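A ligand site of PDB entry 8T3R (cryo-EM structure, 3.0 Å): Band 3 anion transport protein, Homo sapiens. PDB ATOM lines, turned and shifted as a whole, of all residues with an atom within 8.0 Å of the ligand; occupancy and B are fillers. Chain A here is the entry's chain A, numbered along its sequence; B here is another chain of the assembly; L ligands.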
ATOM      1  N   LEU A 811      -4.060   6.475   2.935  1.00  0.00           N
ATOM      2  CA  LEU A 811      -4.765   7.674   3.369  1.00  0.00           C
ATOM      3  C   LEU A 811      -4.850   8.744   2.295  1.00  0.00           C
ATOM      4  O   LEU A 811      -5.617   9.698   2.472  1.00  0.00           O
ATOM      5  CB  LEU A 811      -4.095   8.265   4.609  1.00  0.00           C
ATOM      6  CG  LEU A 811      -4.493   7.625   5.938  1.00  0.00           C
ATOM      7  CD1 LEU A 811      -3.966   8.461   7.094  1.00  0.00           C
ATOM      8  CD2 LEU A 811      -5.995   7.484   6.019  1.00  0.00           C
ATOM      9  N   LEU A 812      -4.073   8.634   1.211  1.00  0.00           N
ATOM     10  CA  LEU A 812      -4.263   9.548   0.079  1.00  0.00           C
ATOM     11  C   LEU A 812      -5.632   9.395  -0.555  1.00  0.00           C
ATOM     12  O   LEU A 812      -6.250  10.389  -0.948  1.00  0.00           O
ATOM     13  CB  LEU A 812      -3.179   9.338  -0.972  1.00  0.00           C
ATOM     14  CG  LEU A 812      -1.994  10.302  -0.984  1.00  0.00           C
ATOM     15  CD1 LEU A 812      -1.103  10.105   0.197  1.00  0.00           C
ATOM     16  CD2 LEU A 812      -1.203  10.126  -2.265  1.00  0.00           C
ATOM     17  N   PHE A 813      -6.128   8.167  -0.665  1.00  0.00           N
ATOM     18  CA  PHE A 813      -7.371   7.907  -1.387  1.00  0.00           C
ATOM     19  C   PHE A 813      -8.620   8.053  -0.531  1.00  0.00           C
ATOM     20  O   PHE A 813      -9.719   8.165  -1.084  1.00  0.00           O
ATOM     21  CB  PHE A 813      -7.329   6.508  -2.002  1.00  0.00           C
ATOM     22  CG  PHE A 813      -6.158   6.297  -2.915  1.00  0.00           C
ATOM     23  CD1 PHE A 813      -6.138   6.864  -4.172  1.00  0.00           C
ATOM     24  CD2 PHE A 813      -5.070   5.553  -2.503  1.00  0.00           C
ATOM     25  CE1 PHE A 813      -5.060   6.684  -5.012  1.00  0.00           C
ATOM     26  CE2 PHE A 813      -3.990   5.365  -3.338  1.00  0.00           C
ATOM     27  CZ  PHE A 813      -3.991   5.932  -4.588  1.00  0.00           C
ATOM     28  N   LYS A 814      -8.486   8.057   0.790  1.00  0.00           N
ATOM     29  CA  LYS A 814      -9.637   8.225   1.651  1.00  0.00           C
ATOM     30  C   LYS A 814     -10.038   9.697   1.747  1.00  0.00           C
ATOM     31  O   LYS A 814      -9.206  10.590   1.548  1.00  0.00           O
ATOM     32  CB  LYS A 814      -9.330   7.694   3.047  1.00  0.00           C
ATOM     33  CG  LYS A 814      -9.165   6.195   3.124  1.00  0.00           C
ATOM     34  CD  LYS A 814      -8.971   5.749   4.555  1.00  0.00           C
ATOM     35  CE  LYS A 814      -8.616   4.278   4.637  1.00  0.00           C
ATOM     36  NZ  LYS A 814      -8.321   3.864   6.031  1.00  0.00           N
ATOM     37  N   PRO A 815     -11.308   9.974   2.022  1.00  0.00           N
ATOM     38  CA  PRO A 815     -11.704  11.339   2.378  1.00  0.00           C
ATOM     39  C   PRO A 815     -11.099  11.747   3.709  1.00  0.00           C
ATOM     40  O   PRO A 815     -10.810  10.880   4.553  1.00  0.00           O
ATOM     41  CB  PRO A 815     -13.233  11.257   2.463  1.00  0.00           C
ATOM     42  CG  PRO A 815     -13.592  10.056   1.678  1.00  0.00           C
ATOM     43  CD  PRO A 815     -12.473   9.100   1.853  1.00  0.00           C
ATOM     44  N   PRO A 816     -10.883  13.051   3.941  1.00  0.00           N
ATOM     45  CA  PRO A 816     -10.266  13.485   5.199  1.00  0.00           C
ATOM     46  C   PRO A 816     -11.085  13.184   6.447  1.00  0.00           C
ATOM     47  O   PRO A 816     -10.516  13.169   7.538  1.00  0.00           O
ATOM     48  CB  PRO A 816     -10.104  15.000   4.996  1.00  0.00           C
ATOM     49  CG  PRO A 816     -10.092  15.187   3.519  1.00  0.00           C
ATOM     50  CD  PRO A 816     -11.036  14.158   2.980  1.00  0.00           C
ATOM     51  N   LYS A 817     -12.384  12.946   6.322  1.00  0.00           N
ATOM     52  CA  LYS A 817     -13.203  12.619   7.477  1.00  0.00           C
ATOM     53  C   LYS A 817     -13.045  11.180   7.938  1.00  0.00           C
ATOM     54  O   LYS A 817     -13.516  10.840   9.027  1.00  0.00           O
ATOM     55  CB  LYS A 817     -14.672  12.908   7.187  1.00  0.00           C
ATOM     56  CG  LYS A 817     -15.263  12.048   6.086  1.00  0.00           C
ATOM     57  CD  LYS A 817     -16.769  12.221   5.999  1.00  0.00           C
ATOM     58  CE  LYS A 817     -17.477  11.456   7.103  1.00  0.00           C
ATOM     59  NZ  LYS A 817     -18.955  11.496   6.937  1.00  0.00           N
ATOM     60  N   TYR A 818     -12.400  10.326   7.144  1.00  0.00           N
ATOM     61  CA  TYR A 818     -12.186   8.926   7.502  1.00  0.00           C
ATOM     62  C   TYR A 818     -10.765   8.646   7.965  1.00  0.00           C
ATOM     63  O   TYR A 818     -10.422   7.480   8.197  1.00  0.00           O
ATOM     64  CB  TYR A 818     -12.542   8.012   6.325  1.00  0.00           C
ATOM     65  CG  TYR A 818     -14.008   7.976   6.003  1.00  0.00           C
ATOM     66  CD1 TYR A 818     -14.906   7.307   6.832  1.00  0.00           C
ATOM     67  CD2 TYR A 818     -14.505   8.602   4.877  1.00  0.00           C
ATOM     68  CE1 TYR A 818     -16.251   7.271   6.548  1.00  0.00           C
ATOM     69  CE2 TYR A 818     -15.859   8.566   4.577  1.00  0.00           C
ATOM     70  CZ  TYR A 818     -16.717   7.900   5.417  1.00  0.00           C
ATOM     71  OH  TYR A 818     -18.064   7.871   5.127  1.00  0.00           O
ATOM     72  N   HIS A 819      -9.920   9.672   8.089  1.00  0.00           N
ATOM     73  CA  HIS A 819      -8.560   9.467   8.536  1.00  0.00           C
ATOM     74  C   HIS A 819      -8.553   9.066  10.015  1.00  0.00           C
ATOM     75  O   HIS A 819      -9.400   9.537  10.786  1.00  0.00           O
ATOM     76  CB  HIS A 819      -7.730  10.737   8.337  1.00  0.00           C
ATOM     77  CG  HIS A 819      -7.553  11.132   6.906  1.00  0.00           C
ATOM     78  ND1 HIS A 819      -7.934  10.321   5.854  1.00  0.00           N
ATOM     79  CD2 HIS A 819      -7.029  12.247   6.344  1.00  0.00           C
ATOM     80  CE1 HIS A 819      -7.657  10.928   4.712  1.00  0.00           C
ATOM     81  NE2 HIS A 819      -7.104  12.095   4.986  1.00  0.00           N
ATOM     82  N   HIS A 834       0.059  14.962   2.910  1.00  0.00           N
ATOM     83  CA  HIS A 834       0.023  14.503   1.519  1.00  0.00           C
ATOM     84  C   HIS A 834       1.274  14.926   0.767  1.00  0.00           C
ATOM     85  O   HIS A 834       1.783  14.154  -0.047  1.00  0.00           O
ATOM     86  CB  HIS A 834      -1.228  15.028   0.827  1.00  0.00           C
ATOM     87  CG  HIS A 834      -2.458  14.229   1.136  1.00  0.00           C
ATOM     88  ND1 HIS A 834      -3.708  14.572   0.663  1.00  0.00           N
ATOM     89  CD2 HIS A 834      -2.633  13.098   1.865  1.00  0.00           C
ATOM     90  CE1 HIS A 834      -4.595  13.689   1.094  1.00  0.00           C
ATOM     91  NE2 HIS A 834      -3.966  12.787   1.823  1.00  0.00           N
ATOM     92  N   SER B 594     -16.548   0.026   1.861  1.00  0.00           N
ATOM     93  CA  SER B 594     -15.275   0.509   2.361  1.00  0.00           C
ATOM     94  C   SER B 594     -15.351   2.009   2.625  1.00  0.00           C
ATOM     95  O   SER B 594     -16.391   2.647   2.461  1.00  0.00           O
ATOM     96  CB  SER B 594     -14.159   0.190   1.375  1.00  0.00           C
ATOM     97  OG  SER B 594     -14.254   1.000   0.225  1.00  0.00           O
ATOM     98  N   SER B 595     -14.229   2.581   3.048  1.00  0.00           N
ATOM     99  CA  SER B 595     -14.128   4.005   3.329  1.00  0.00           C
ATOM    100  C   SER B 595     -13.319   4.758   2.288  1.00  0.00           C
ATOM    101  O   SER B 595     -13.150   5.977   2.424  1.00  0.00           O
ATOM    102  CB  SER B 595     -13.506   4.218   4.710  1.00  0.00           C
ATOM    103  OG  SER B 595     -12.277   3.527   4.832  1.00  0.00           O
ATOM    104  N   TYR B 596     -12.818   4.083   1.255  1.00  0.00           N
ATOM    105  CA  TYR B 596     -12.017   4.739   0.235  1.00  0.00           C
ATOM    106  C   TYR B 596     -12.907   5.524  -0.722  1.00  0.00           C
ATOM    107  O   TYR B 596     -14.123   5.327  -0.773  1.00  0.00           O
ATOM    108  CB  TYR B 596     -11.200   3.714  -0.537  1.00  0.00           C
ATOM    109  CG  TYR B 596     -10.204   2.977   0.314  1.00  0.00           C
ATOM    110  CD1 TYR B 596      -8.943   3.509   0.563  1.00  0.00           C
ATOM    111  CD2 TYR B 596     -10.511   1.754   0.888  1.00  0.00           C
ATOM    112  CE1 TYR B 596      -8.031   2.844   1.345  1.00  0.00           C
ATOM    113  CE2 TYR B 596      -9.608   1.078   1.674  1.00  0.00           C
ATOM    114  CZ  TYR B 596      -8.367   1.624   1.896  1.00  0.00           C
ATOM    115  OH  TYR B 596      -7.456   0.959   2.677  1.00  0.00           O
ATOM    116  N   PHE B 597     -12.279   6.464  -1.448  1.00  0.00           N
ATOM    117  CA  PHE B 597     -12.829   7.262  -2.538  1.00  0.00           C
ATOM    118  C   PHE B 597     -13.905   8.229  -2.053  1.00  0.00           C
ATOM    119  O   PHE B 597     -14.307   8.156  -0.875  1.00  0.00           O
ATOM    120  CB  PHE B 597     -13.379   6.333  -3.644  1.00  0.00           C
ATOM    121  CG  PHE B 597     -12.370   5.979  -4.690  1.00  0.00           C
ATOM    122  CD1 PHE B 597     -11.109   5.544  -4.339  1.00  0.00           C
ATOM    123  CD2 PHE B 597     -12.689   6.088  -6.040  1.00  0.00           C
ATOM    124  CE1 PHE B 597     -10.181   5.215  -5.304  1.00  0.00           C
ATOM    125  CE2 PHE B 597     -11.761   5.759  -7.005  1.00  0.00           C
ATOM    126  CZ  PHE B 597     -10.503   5.327  -6.633  1.00  0.00           C
ATOM    127  N   PRO B 598     -14.368   9.178  -2.868  1.00  0.00           N
ATOM    128  CA  PRO B 598     -15.574   9.926  -2.509  1.00  0.00           C
ATOM    129  C   PRO B 598     -16.765   8.991  -2.359  1.00  0.00           C
ATOM    130  O   PRO B 598     -16.861   7.965  -3.049  1.00  0.00           O
ATOM    131  CB  PRO B 598     -15.759  10.881  -3.689  1.00  0.00           C
ATOM    132  CG  PRO B 598     -14.393  11.114  -4.194  1.00  0.00           C
ATOM    133  CD  PRO B 598     -13.612   9.842  -3.956  1.00  0.00           C
ATOM    134  N   GLY B 599     -17.672   9.347  -1.451  1.00  0.00           N
ATOM    135  CA  GLY B 599     -18.767   8.462  -1.108  1.00  0.00           C
ATOM    136  C   GLY B 599     -19.707   8.192  -2.263  1.00  0.00           C
ATOM    137  O   GLY B 599     -20.167   7.069  -2.462  1.00  0.00           O
ATOM    138  N   LYS B 600     -20.015   9.243  -3.044  1.00  0.00           N
ATOM    139  CA  LYS B 600     -20.888   9.070  -4.200  1.00  0.00           C
ATOM    140  C   LYS B 600     -20.239   8.183  -5.264  1.00  0.00           C
ATOM    141  O   LYS B 600     -20.870   7.267  -5.799  1.00  0.00           O
ATOM    142  CB  LYS B 600     -21.249  10.434  -4.788  1.00  0.00           C
ATOM    143  CG  LYS B 600     -22.093  11.298  -3.867  1.00  0.00           C
ATOM    144  CD  LYS B 600     -22.588  12.535  -4.588  1.00  0.00           C
ATOM    145  CE  LYS B 600     -23.390  13.431  -3.649  1.00  0.00           C
ATOM    146  NZ  LYS B 600     -23.790  14.706  -4.304  1.00  0.00           N
ATOM    147  N   LEU B 601     -18.960   8.434  -5.553  1.00  0.00           N
ATOM    148  CA  LEU B 601     -18.238   7.619  -6.530  1.00  0.00           C
ATOM    149  C   LEU B 601     -18.068   6.189  -6.022  1.00  0.00           C
ATOM    150  O   LEU B 601     -18.153   5.239  -6.802  1.00  0.00           O
ATOM    151  CB  LEU B 601     -16.885   8.245  -6.842  1.00  0.00           C
ATOM    152  CG  LEU B 601     -16.373   8.050  -8.271  1.00  0.00           C
ATOM    153  CD1 LEU B 601     -17.440   8.450  -9.278  1.00  0.00           C
ATOM    154  CD2 LEU B 601     -15.094   8.826  -8.503  1.00  0.00           C
ATOM    155  N   ARG B 602     -17.834   6.032  -4.717  1.00  0.00           N
ATOM    156  CA  ARG B 602     -17.722   4.698  -4.140  1.00  0.00           C
ATOM    157  C   ARG B 602     -19.036   3.928  -4.273  1.00  0.00           C
ATOM    158  O   ARG B 602     -19.027   2.747  -4.643  1.00  0.00           O
ATOM    159  CB  ARG B 602     -17.320   4.793  -2.671  1.00  0.00           C
ATOM    160  CG  ARG B 602     -17.322   3.487  -1.927  1.00  0.00           C
ATOM    161  CD  ARG B 602     -17.545   3.709  -0.450  1.00  0.00           C
ATOM    162  NE  ARG B 602     -16.923   4.947   0.020  1.00  0.00           N
ATOM    163  CZ  ARG B 602     -17.156   5.493   1.201  1.00  0.00           C
ATOM    164  NH1 ARG B 602     -17.976   4.939   2.070  1.00  0.00           N
ATOM    165  NH2 ARG B 602     -16.536   6.627   1.516  1.00  0.00           N
ATOM    166  N   ARG B 603     -20.161   4.587  -4.016  1.00  0.00           N
ATOM    167  CA  ARG B 603     -21.461   3.911  -4.141  1.00  0.00           C
ATOM    168  C   ARG B 603     -21.781   3.597  -5.598  1.00  0.00           C
ATOM    169  O   ARG B 603     -22.363   2.538  -5.885  1.00  0.00           O
ATOM    170  CB  ARG B 603     -22.565   4.765  -3.524  1.00  0.00           C
ATOM    171  CG  ARG B 603     -22.489   4.877  -2.008  1.00  0.00           C
ATOM    172  CD  ARG B 603     -22.711   3.531  -1.333  1.00  0.00           C
ATOM    173  NE  ARG B 603     -23.054   3.693   0.071  1.00  0.00           N
ATOM    174  CZ  ARG B 603     -22.169   3.686   1.062  1.00  0.00           C
ATOM    175  NH1 ARG B 603     -20.880   3.503   0.833  1.00  0.00           N
ATOM    176  NH2 ARG B 603     -22.590   3.864   2.312  1.00  0.00           N
HETATM  177  C1  LIG L   1     -16.545  14.665   1.636  1.00  0.00           C
HETATM  178  O1  LIG L   1     -16.152  15.617   0.685  1.00  0.00           O
HETATM  179  P1  LIG L   1     -14.576  16.089   0.680  1.00  0.00           P
HETATM  180  C2  LIG L   1     -16.360  13.269   1.040  1.00  0.00           C
HETATM  181  O2  LIG L   1     -17.037  13.218  -0.191  1.00  0.00           O
HETATM  182  C3  LIG L   1     -16.904  12.165   1.952  1.00  0.00           C
HETATM  183  O3  LIG L   1     -16.838  10.940   1.264  1.00  0.00           O
HETATM  184  C4  LIG L   1     -18.357  12.429   2.371  1.00  0.00           C
HETATM  185  O4  LIG L   1     -18.754  11.456   3.310  1.00  0.00           O
HETATM  186  P2  LIG L   1     -19.559  10.124   2.768  1.00  0.00           P
HETATM  187  C5  LIG L   1     -18.523  13.819   2.989  1.00  0.00           C
HETATM  188  O5  LIG L   1     -19.882  14.036   3.272  1.00  0.00           O
HETATM  189  P3  LIG L   1     -20.335  14.213   4.839  1.00  0.00           P
HETATM  190  C6  LIG L   1     -18.006  14.922   2.045  1.00  0.00           C
HETATM  191  O6  LIG L   1     -18.101  16.161   2.692  1.00  0.00           O
HETATM  192  O7  LIG L   1     -14.034  16.052   2.091  1.00  0.00           O
HETATM  193  O8  LIG L   1     -14.461  17.497   0.128  1.00  0.00           O
HETATM  194  O9  LIG L   1     -13.685  15.072  -0.267  1.00  0.00           O
HETATM  195  C7  LIG L   1     -11.857  13.037  -1.734  1.00  0.00           C
HETATM  196  O10 LIG L   1     -12.151  12.572  -0.684  1.00  0.00           O
HETATM  197  C8  LIG L   1     -11.820  15.138  -5.936  1.00  0.00           C
HETATM  198  O11 LIG L   1     -12.781  15.487  -6.540  1.00  0.00           O
HETATM  199  C9  LIG L   1     -12.859  15.622  -1.252  1.00  0.00           C
HETATM  200  C10 LIG L   1     -10.394  13.006  -2.171  1.00  0.00           C
HETATM  201  C11 LIG L   1     -10.446  15.195  -6.598  1.00  0.00           C
HETATM  202  C12 LIG L   1     -13.143  14.937  -2.582  1.00  0.00           C
HETATM  203  O12 LIG L   1     -12.844  13.557  -2.584  1.00  0.00           O
HETATM  204  C13 LIG L   1      -9.939  11.552  -2.165  1.00  0.00           C
HETATM  205  C14 LIG L   1     -12.391  15.640  -3.719  1.00  0.00           C
HETATM  206  O13 LIG L   1     -11.949  14.670  -4.627  1.00  0.00           O
HETATM  207  O14 LIG L   1     -20.256  10.466   1.475  1.00  0.00           O
HETATM  208  O15 LIG L   1     -18.562   9.019   2.536  1.00  0.00           O
HETATM  209  O16 LIG L   1     -20.572   9.696   3.791  1.00  0.00           O
HETATM  210  C15 LIG L   1      -9.014  11.310  -3.365  1.00  0.00           C
HETATM  211  O17 LIG L   1     -20.907  12.917   5.363  1.00  0.00           O
HETATM  212  O18 LIG L   1     -19.144  14.608   5.669  1.00  0.00           O
HETATM  213  O19 LIG L   1     -21.388  15.294   4.923  1.00  0.00           O
HETATM  214  C16 LIG L   1      -9.778  10.577  -4.463  1.00  0.00           C
HETATM  215  C17 LIG L   1      -8.782  10.080  -5.499  1.00  0.00           C
HETATM  216  C18 LIG L   1      -9.476   9.100  -6.438  1.00  0.00           C
HETATM  217  C19 LIG L   1      -8.667   8.978  -7.734  1.00  0.00           C
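An oxygen (O15) of the ligand is in salt-bridge range of the guanidinium group of Arg 602 of chain B, at 3.3 Å.
N of Gly 599 of chain B lies within hydrogen-bond range of O3 of the ligand (3.3 Å).
The side-chain hydroxyl of Tyr 818 lies within hydrogen-bond range of an oxygen (O15) of the ligand (2.9 Å).
The side-chain amino group of Lys 817 is in salt-bridge range of an oxygen (O17) of the ligand (2.9 Å).
N of Phe 597 of chain B sits at hydrogen-bond distance from O of Phe 813 (3.1 Å).
The backbone carbonyl oxygen (O) of Pro 815 sits close to a ring nitrogen (ND1) of His 819 (3.2 Å).
NH1 of Arg 602 of chain B is in hydrogen-bond range of O of Ser 594 of chain B, 2.8 Å away.
NE of Arg 602 of chain B lies within hydrogen-bond range of O of Tyr 596 of chain B (2.9 Å).
Residues that only touch the ligand: Pro 598 of chain B, Pro 815, Phe 813, Pro 816, Leu 812, Lys 814 and Phe 597 of chain B.
Hydrophobic or aromatic side chains within 4 Å of the ligand: Pro 815, Pro 816, Tyr 818, Phe 597 of chain B and Pro 598 of chain B.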
